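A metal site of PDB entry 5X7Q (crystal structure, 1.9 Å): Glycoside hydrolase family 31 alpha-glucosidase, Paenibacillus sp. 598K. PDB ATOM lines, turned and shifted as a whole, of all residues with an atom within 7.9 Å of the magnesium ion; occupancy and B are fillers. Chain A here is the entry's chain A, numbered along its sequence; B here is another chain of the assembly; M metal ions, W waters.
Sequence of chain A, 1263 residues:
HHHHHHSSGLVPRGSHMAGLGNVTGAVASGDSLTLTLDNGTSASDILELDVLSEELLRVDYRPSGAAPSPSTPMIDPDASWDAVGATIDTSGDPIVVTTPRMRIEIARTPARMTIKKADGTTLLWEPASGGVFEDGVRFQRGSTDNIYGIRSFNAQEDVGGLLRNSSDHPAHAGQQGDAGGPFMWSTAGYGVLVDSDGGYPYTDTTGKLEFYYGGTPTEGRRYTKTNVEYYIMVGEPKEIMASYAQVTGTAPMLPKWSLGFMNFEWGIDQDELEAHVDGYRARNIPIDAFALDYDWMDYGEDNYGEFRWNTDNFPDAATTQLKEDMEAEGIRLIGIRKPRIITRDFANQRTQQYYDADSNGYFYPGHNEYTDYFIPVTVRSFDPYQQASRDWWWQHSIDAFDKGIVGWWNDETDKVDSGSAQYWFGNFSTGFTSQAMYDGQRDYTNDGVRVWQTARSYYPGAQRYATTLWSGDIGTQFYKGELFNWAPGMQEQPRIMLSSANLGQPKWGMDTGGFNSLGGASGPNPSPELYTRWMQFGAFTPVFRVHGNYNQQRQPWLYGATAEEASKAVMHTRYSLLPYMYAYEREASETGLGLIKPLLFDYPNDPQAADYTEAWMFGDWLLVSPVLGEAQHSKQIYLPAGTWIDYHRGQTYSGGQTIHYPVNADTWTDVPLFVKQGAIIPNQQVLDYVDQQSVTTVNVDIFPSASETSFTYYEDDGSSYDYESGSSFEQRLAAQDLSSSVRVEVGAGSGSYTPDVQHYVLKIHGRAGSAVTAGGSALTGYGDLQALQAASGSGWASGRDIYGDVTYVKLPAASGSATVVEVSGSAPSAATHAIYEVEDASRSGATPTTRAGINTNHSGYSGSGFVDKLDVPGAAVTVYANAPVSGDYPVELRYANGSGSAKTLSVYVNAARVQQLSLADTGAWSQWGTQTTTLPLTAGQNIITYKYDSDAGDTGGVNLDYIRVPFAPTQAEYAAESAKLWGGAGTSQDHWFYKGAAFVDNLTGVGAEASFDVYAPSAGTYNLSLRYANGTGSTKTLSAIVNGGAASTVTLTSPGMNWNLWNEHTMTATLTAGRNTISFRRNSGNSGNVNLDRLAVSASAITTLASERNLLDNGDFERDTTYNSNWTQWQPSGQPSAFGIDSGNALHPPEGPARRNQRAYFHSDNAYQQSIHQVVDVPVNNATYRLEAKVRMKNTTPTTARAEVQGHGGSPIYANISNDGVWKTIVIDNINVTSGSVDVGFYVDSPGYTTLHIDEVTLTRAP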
ATOM      1  N   PHE A 264     -10.627  -2.473 -21.526  1.00  0.00           N
ATOM      2  CA  PHE A 264     -10.592  -2.658 -20.064  1.00  0.00           C
ATOM      3  C   PHE A 264     -11.697  -3.646 -19.711  1.00  0.00           C
ATOM      4  O   PHE A 264     -12.784  -3.597 -20.300  1.00  0.00           O
ATOM      5  CB  PHE A 264     -10.800  -1.345 -19.306  1.00  0.00           C
ATOM      6  CG  PHE A 264      -9.571  -0.465 -19.279  1.00  0.00           C
ATOM      7  CD1 PHE A 264      -8.936  -0.097 -20.455  1.00  0.00           C
ATOM      8  CD2 PHE A 264      -9.046  -0.007 -18.073  1.00  0.00           C
ATOM      9  CE1 PHE A 264      -7.775   0.689 -20.433  1.00  0.00           C
ATOM     10  CE2 PHE A 264      -7.907   0.795 -18.030  1.00  0.00           C
ATOM     11  CZ  PHE A 264      -7.270   1.145 -19.219  1.00  0.00           C
ATOM     12  N   GLU A 265     -11.424  -4.572 -18.791  1.00  0.00           N
ATOM     13  CA  GLU A 265     -12.460  -5.529 -18.424  1.00  0.00           C
ATOM     14  C   GLU A 265     -12.324  -6.019 -16.992  1.00  0.00           C
ATOM     15  O   GLU A 265     -11.217  -6.308 -16.530  1.00  0.00           O
ATOM     16  CB  GLU A 265     -12.456  -6.731 -19.386  1.00  0.00           C
ATOM     17  CG  GLU A 265     -13.721  -7.580 -19.267  1.00  0.00           C
ATOM     18  CD  GLU A 265     -13.922  -8.547 -20.448  1.00  0.00           C
ATOM     19  OE1 GLU A 265     -13.673  -8.141 -21.603  1.00  0.00           O
ATOM     20  OE2 GLU A 265     -14.386  -9.694 -20.217  1.00  0.00           O
ATOM     21  N   TRP A 266     -13.465  -6.150 -16.331  1.00  0.00           N
ATOM     22  CA  TRP A 266     -13.604  -6.744 -15.018  1.00  0.00           C
ATOM     23  C   TRP A 266     -14.510  -7.975 -15.153  1.00  0.00           C
ATOM     24  O   TRP A 266     -15.654  -7.866 -15.592  1.00  0.00           O
ATOM     25  CB  TRP A 266     -14.244  -5.697 -14.098  1.00  0.00           C
ATOM     26  CG  TRP A 266     -14.392  -6.090 -12.664  1.00  0.00           C
ATOM     27  CD1 TRP A 266     -13.795  -7.143 -12.013  1.00  0.00           C
ATOM     28  CD2 TRP A 266     -15.148  -5.397 -11.682  1.00  0.00           C
ATOM     29  NE1 TRP A 266     -14.153  -7.146 -10.697  1.00  0.00           N
ATOM     30  CE2 TRP A 266     -15.003  -6.091 -10.462  1.00  0.00           C
ATOM     31  CE3 TRP A 266     -15.971  -4.257 -11.724  1.00  0.00           C
ATOM     32  CZ2 TRP A 266     -15.631  -5.673  -9.286  1.00  0.00           C
ATOM     33  CZ3 TRP A 266     -16.597  -3.847 -10.559  1.00  0.00           C
ATOM     34  CH2 TRP A 266     -16.421  -4.548  -9.348  1.00  0.00           C
ATOM     35  N   GLY A 267     -13.973  -9.132 -14.774  1.00  0.00           N
ATOM     36  CA  GLY A 267     -14.623 -10.420 -15.028  1.00  0.00           C
ATOM     37  C   GLY A 267     -13.984 -11.030 -16.262  1.00  0.00           C
ATOM     38  O   GLY A 267     -14.536 -10.960 -17.357  1.00  0.00           O
ATOM     39  N   ILE A 268     -12.819 -11.620 -16.078  1.00  0.00           N
ATOM     40  CA  ILE A 268     -11.987 -12.060 -17.188  1.00  0.00           C
ATOM     41  C   ILE A 268     -10.928 -13.017 -16.656  1.00  0.00           C
ATOM     42  O   ILE A 268     -10.340 -12.768 -15.618  1.00  0.00           O
ATOM     43  CB  ILE A 268     -11.341 -10.847 -17.931  1.00  0.00           C
ATOM     44  CG1 ILE A 268     -10.613 -11.304 -19.198  1.00  0.00           C
ATOM     45  CG2 ILE A 268     -10.415 -10.062 -17.001  1.00  0.00           C
ATOM     46  CD1 ILE A 268     -10.342 -10.186 -20.181  1.00  0.00           C
ATOM     47  N   ASP A 269     -10.712 -14.125 -17.363  1.00  0.00           N
ATOM     48  CA  ASP A 269      -9.609 -15.043 -17.076  1.00  0.00           C
ATOM     49  C   ASP A 269      -8.814 -15.300 -18.358  1.00  0.00           C
ATOM     50  O   ASP A 269      -9.126 -14.701 -19.388  1.00  0.00           O
ATOM     51  CB  ASP A 269     -10.142 -16.334 -16.429  1.00  0.00           C
ATOM     52  CG  ASP A 269     -11.027 -17.159 -17.353  1.00  0.00           C
ATOM     53  OD1 ASP A 269     -11.203 -16.837 -18.556  1.00  0.00           O
ATOM     54  OD2 ASP A 269     -11.543 -18.167 -16.853  1.00  0.00           O
ATOM     55  N   GLU A 272     -10.728 -16.493 -21.574  1.00  0.00           N
ATOM     56  CA  GLU A 272     -11.607 -15.454 -22.113  1.00  0.00           C
ATOM     57  C   GLU A 272     -10.822 -14.345 -22.812  1.00  0.00           C
ATOM     58  O   GLU A 272     -11.237 -13.865 -23.885  1.00  0.00           O
ATOM     59  CB  GLU A 272     -12.521 -14.891 -21.028  1.00  0.00           C
ATOM     60  CG  GLU A 272     -13.532 -15.896 -20.505  1.00  0.00           C
ATOM     61  CD  GLU A 272     -14.194 -15.476 -19.189  1.00  0.00           C
ATOM     62  OE1 GLU A 272     -13.992 -14.327 -18.749  1.00  0.00           O
ATOM     63  OE2 GLU A 272     -14.944 -16.295 -18.614  1.00  0.00           O
ATOM     64  N   LEU A 273      -9.710 -13.938 -22.203  1.00  0.00           N
ATOM     65  CA  LEU A 273      -8.781 -12.985 -22.796  1.00  0.00           C
ATOM     66  C   LEU A 273      -8.312 -13.454 -24.172  1.00  0.00           C
ATOM     67  O   LEU A 273      -8.346 -12.672 -25.128  1.00  0.00           O
ATOM     68  CB  LEU A 273      -7.587 -12.736 -21.872  1.00  0.00           C
ATOM     69  CG  LEU A 273      -6.438 -11.892 -22.423  1.00  0.00           C
ATOM     70  CD1 LEU A 273      -6.870 -10.468 -22.730  1.00  0.00           C
ATOM     71  CD2 LEU A 273      -5.247 -11.899 -21.488  1.00  0.00           C
ATOM     72  N   HIS A 276     -11.163 -13.187 -26.622  1.00  0.00           N
ATOM     73  CA  HIS A 276     -11.366 -11.769 -26.999  1.00  0.00           C
ATOM     74  C   HIS A 276     -10.346 -11.329 -28.031  1.00  0.00           C
ATOM     75  O   HIS A 276     -10.716 -10.793 -29.068  1.00  0.00           O
ATOM     76  CB  HIS A 276     -11.297 -10.791 -25.808  1.00  0.00           C
ATOM     77  CG  HIS A 276     -12.297 -11.055 -24.730  1.00  0.00           C
ATOM     78  ND1 HIS A 276     -13.513 -11.652 -24.956  1.00  0.00           N
ATOM     79  CD2 HIS A 276     -12.262 -10.777 -23.403  1.00  0.00           C
ATOM     80  CE1 HIS A 276     -14.171 -11.758 -23.823  1.00  0.00           C
ATOM     81  NE2 HIS A 276     -13.432 -11.243 -22.862  1.00  0.00           N
ATOM     82  N   PHE A 290      -5.133  -4.854 -23.396  1.00  0.00           N
ATOM     83  CA  PHE A 290      -6.198  -5.258 -22.515  1.00  0.00           C
ATOM     84  C   PHE A 290      -5.814  -4.802 -21.119  1.00  0.00           C
ATOM     85  O   PHE A 290      -4.655  -4.913 -20.719  1.00  0.00           O
ATOM     86  CB  PHE A 290      -6.401  -6.779 -22.556  1.00  0.00           C
ATOM     87  CG  PHE A 290      -7.703  -7.193 -23.175  1.00  0.00           C
ATOM     88  CD1 PHE A 290      -8.846  -7.325 -22.402  1.00  0.00           C
ATOM     89  CD2 PHE A 290      -7.775  -7.469 -24.525  1.00  0.00           C
ATOM     90  CE1 PHE A 290     -10.054  -7.683 -22.970  1.00  0.00           C
ATOM     91  CE2 PHE A 290      -8.981  -7.845 -25.107  1.00  0.00           C
ATOM     92  CZ  PHE A 290     -10.115  -7.957 -24.329  1.00  0.00           C
ATOM     93  N   ASP A 295      -9.378  -9.375 -11.308  1.00  0.00           N
ATOM     94  CA  ASP A 295      -9.080 -10.701 -11.865  1.00  0.00           C
ATOM     95  C   ASP A 295      -7.601 -11.025 -11.978  1.00  0.00           C
ATOM     96  O   ASP A 295      -7.226 -12.186 -11.779  1.00  0.00           O
ATOM     97  CB  ASP A 295      -9.716 -10.875 -13.252  1.00  0.00           C
ATOM     98  CG  ASP A 295     -11.131 -10.392 -13.317  1.00  0.00           C
ATOM     99  OD1 ASP A 295     -11.335  -9.176 -13.437  1.00  0.00           O
ATOM    100  OD2 ASP A 295     -12.067 -11.221 -13.274  1.00  0.00           O
ATOM    101  N   ASN B 348     -20.946 -16.379 -12.925  1.00  0.00           N
ATOM    102  CA  ASN B 348     -21.884 -15.620 -13.781  1.00  0.00           C
ATOM    103  C   ASN B 348     -22.961 -16.450 -14.510  1.00  0.00           C
ATOM    104  O   ASN B 348     -23.537 -15.988 -15.479  1.00  0.00           O
ATOM    105  CB  ASN B 348     -21.144 -14.702 -14.767  1.00  0.00           C
ATOM    106  CG  ASN B 348     -21.987 -13.517 -15.212  1.00  0.00           C
ATOM    107  OD1 ASN B 348     -22.654 -12.880 -14.396  1.00  0.00           O
ATOM    108  ND2 ASN B 348     -21.992 -13.220 -16.506  1.00  0.00           N
ATOM    109  N   ASN B 549     -18.923  -2.555 -16.115  1.00  0.00           N
ATOM    110  CA  ASN B 549     -19.029  -3.084 -14.754  1.00  0.00           C
ATOM    111  C   ASN B 549     -18.696  -4.582 -14.728  1.00  0.00           C
ATOM    112  O   ASN B 549     -18.410  -5.186 -15.760  1.00  0.00           O
ATOM    113  CB  ASN B 549     -20.424  -2.803 -14.182  1.00  0.00           C
ATOM    114  CG  ASN B 549     -20.418  -2.518 -12.682  1.00  0.00           C
ATOM    115  OD1 ASN B 549     -19.603  -3.066 -11.951  1.00  0.00           O
ATOM    116  ND2 ASN B 549     -21.355  -1.705 -12.216  1.00  0.00           N
ATOM    117  N   TYR B 550     -18.725  -5.138 -13.529  1.00  0.00           N
ATOM    118  CA  TYR B 550     -18.337  -6.520 -13.290  1.00  0.00           C
ATOM    119  C   TYR B 550     -19.100  -7.475 -14.197  1.00  0.00           C
ATOM    120  O   TYR B 550     -20.321  -7.418 -14.275  1.00  0.00           O
ATOM    121  CB  TYR B 550     -18.590  -6.884 -11.820  1.00  0.00           C
ATOM    122  CG  TYR B 550     -18.214  -8.308 -11.468  1.00  0.00           C
ATOM    123  CD1 TYR B 550     -16.909  -8.738 -11.607  1.00  0.00           C
ATOM    124  CD2 TYR B 550     -19.176  -9.231 -11.047  1.00  0.00           C
ATOM    125  CE1 TYR B 550     -16.531 -10.041 -11.303  1.00  0.00           C
ATOM    126  CE2 TYR B 550     -18.820 -10.539 -10.725  1.00  0.00           C
ATOM    127  CZ  TYR B 550     -17.497 -10.928 -10.855  1.00  0.00           C
ATOM    128  OH  TYR B 550     -17.119 -12.210 -10.556  1.00  0.00           O
ATOM    129  N   ASN B 551     -18.346  -8.297 -14.928  1.00  0.00           N
ATOM    130  CA  ASN B 551     -18.893  -9.274 -15.879  1.00  0.00           C
ATOM    131  C   ASN B 551     -19.712  -8.702 -17.056  1.00  0.00           C
ATOM    132  O   ASN B 551     -20.449  -9.442 -17.693  1.00  0.00           O
ATOM    133  CB  ASN B 551     -19.701 -10.380 -15.152  1.00  0.00           C
ATOM    134  CG  ASN B 551     -18.813 -11.474 -14.582  1.00  0.00           C
ATOM    135  OD1 ASN B 551     -17.711 -11.696 -15.059  1.00  0.00           O
ATOM    136  ND2 ASN B 551     -19.301 -12.161 -13.567  1.00  0.00           N
ATOM    137  N   GLN B 552     -19.570  -7.409 -17.332  1.00  0.00           N
ATOM    138  CA  GLN B 552     -20.126  -6.799 -18.537  1.00  0.00           C
ATOM    139  C   GLN B 552     -19.083  -6.895 -19.640  1.00  0.00           C
ATOM    140  O   GLN B 552     -17.872  -6.958 -19.370  1.00  0.00           O
ATOM    141  CB  GLN B 552     -20.516  -5.347 -18.291  1.00  0.00           C
ATOM    142  CG  GLN B 552     -21.577  -5.205 -17.222  1.00  0.00           C
ATOM    143  CD  GLN B 552     -22.214  -3.826 -17.189  1.00  0.00           C
ATOM    144  OE1 GLN B 552     -21.591  -2.828 -17.557  1.00  0.00           O
ATOM    145  NE2 GLN B 552     -23.454  -3.756 -16.693  1.00  0.00           N
ATOM    146  N   GLN B 553     -19.566  -6.957 -20.877  1.00  0.00           N
ATOM    147  CA  GLN B 553     -18.705  -7.131 -22.045  1.00  0.00           C
ATOM    148  C   GLN B 553     -18.845  -5.944 -22.963  1.00  0.00           C
ATOM    149  O   GLN B 553     -19.948  -5.401 -23.150  1.00  0.00           O
ATOM    150  CB  GLN B 553     -19.081  -8.409 -22.813  1.00  0.00           C
ATOM    151  CG  GLN B 553     -18.920  -9.727 -22.062  1.00  0.00           C
ATOM    152  CD  GLN B 553     -17.539  -9.917 -21.461  1.00  0.00           C
ATOM    153  OE1 GLN B 553     -17.434 -10.344 -20.316  1.00  0.00           O
ATOM    154  NE2 GLN B 553     -16.484  -9.589 -22.214  1.00  0.00           N
ATOM    155  N   ARG B 554     -17.729  -5.552 -23.554  1.00  0.00           N
ATOM    156  CA  ARG B 554     -17.674  -4.367 -24.412  1.00  0.00           C
ATOM    157  C   ARG B 554     -17.059  -4.643 -25.798  1.00  0.00           C
ATOM    158  O   ARG B 554     -16.679  -3.712 -26.520  1.00  0.00           O
ATOM    159  CB  ARG B 554     -16.897  -3.254 -23.688  1.00  0.00           C
ATOM    160  CG  ARG B 554     -17.604  -2.708 -22.454  1.00  0.00           C
ATOM    161  CD  ARG B 554     -18.799  -1.821 -22.818  1.00  0.00           C
ATOM    162  NE  ARG B 554     -19.460  -1.261 -21.647  1.00  0.00           N
ATOM    163  CZ  ARG B 554     -20.480  -1.816 -20.976  1.00  0.00           C
ATOM    164  NH1 ARG B 554     -21.011  -2.986 -21.339  1.00  0.00           N
ATOM    165  NH2 ARG B 554     -20.981  -1.176 -19.917  1.00  0.00           N
ATOM    166  N   GLN B 555     -17.000  -5.918 -26.205  1.00  0.00           N
ATOM    167  CA  GLN B 555     -16.470  -6.230 -27.535  1.00  0.00           C
ATOM    168  C   GLN B 555     -17.509  -5.814 -28.590  1.00  0.00           C
ATOM    169  O   GLN B 555     -18.696  -6.078 -28.420  1.00  0.00           O
ATOM    170  CB  GLN B 555     -16.072  -7.705 -27.661  1.00  0.00           C
ATOM    171  CG  GLN B 555     -14.839  -8.097 -26.838  1.00  0.00           C
ATOM    172  CD  GLN B 555     -15.146  -8.353 -25.362  1.00  0.00           C
ATOM    173  OE1 GLN B 555     -16.225  -8.861 -25.005  1.00  0.00           O
ATOM    174  NE2 GLN B 555     -14.211  -7.962 -24.498  1.00  0.00           N
HETATM  175 MG    MG M   1     -15.835 -10.676 -18.965  1.00  0.00          MG
HETATM  176  O   HOH W   1     -16.512  -8.911 -18.082  1.00  0.00           O
HETATM  177  O   HOH W   2     -15.165 -12.361 -20.006  1.00  0.00           O
HETATM  178  O   HOH W   3     -17.140 -11.875 -17.986  1.00  0.00           O
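N of Gly 267 is in hydrogen-bond range of OD1 of Asp 295, at 3.0 Å.
OE1 of Gln 555 of chain B lies within hydrogen-bond range of NE2 of Gln 553 of chain B, 2.9 Å away.
A ring nitrogen (NE2) of His 276 sits at hydrogen-bond distance from the side-chain carboxylate of Glu 265, 3.4 Å away.
The side-chain amide nitrogen (NE2) of Gln 555 of chain B lies within hydrogen-bond range of the side-chain carboxylate (OE1) of Glu 265 (3.0 Å).
The magnesium ion is bound by water W3, 2.0 Å away.
The magnesium ion is bound by water W1, 2.1 Å away.
The magnesium ion is bound by O of Gly 267 (2.1 Å).
Water W2 binds the magnesium ion (2.1 Å).
OE1 of Gln 553 of chain B binds the magnesium ion.
The magnesium ion is bound by OE2 of Glu 265 (2.2 Å).
The magnesium ion has six donor atoms within binding distance.
Water W1 bridges O of Gln 552 of chain B (2.7 Å) and O of Trp 266 (2.8 Å).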
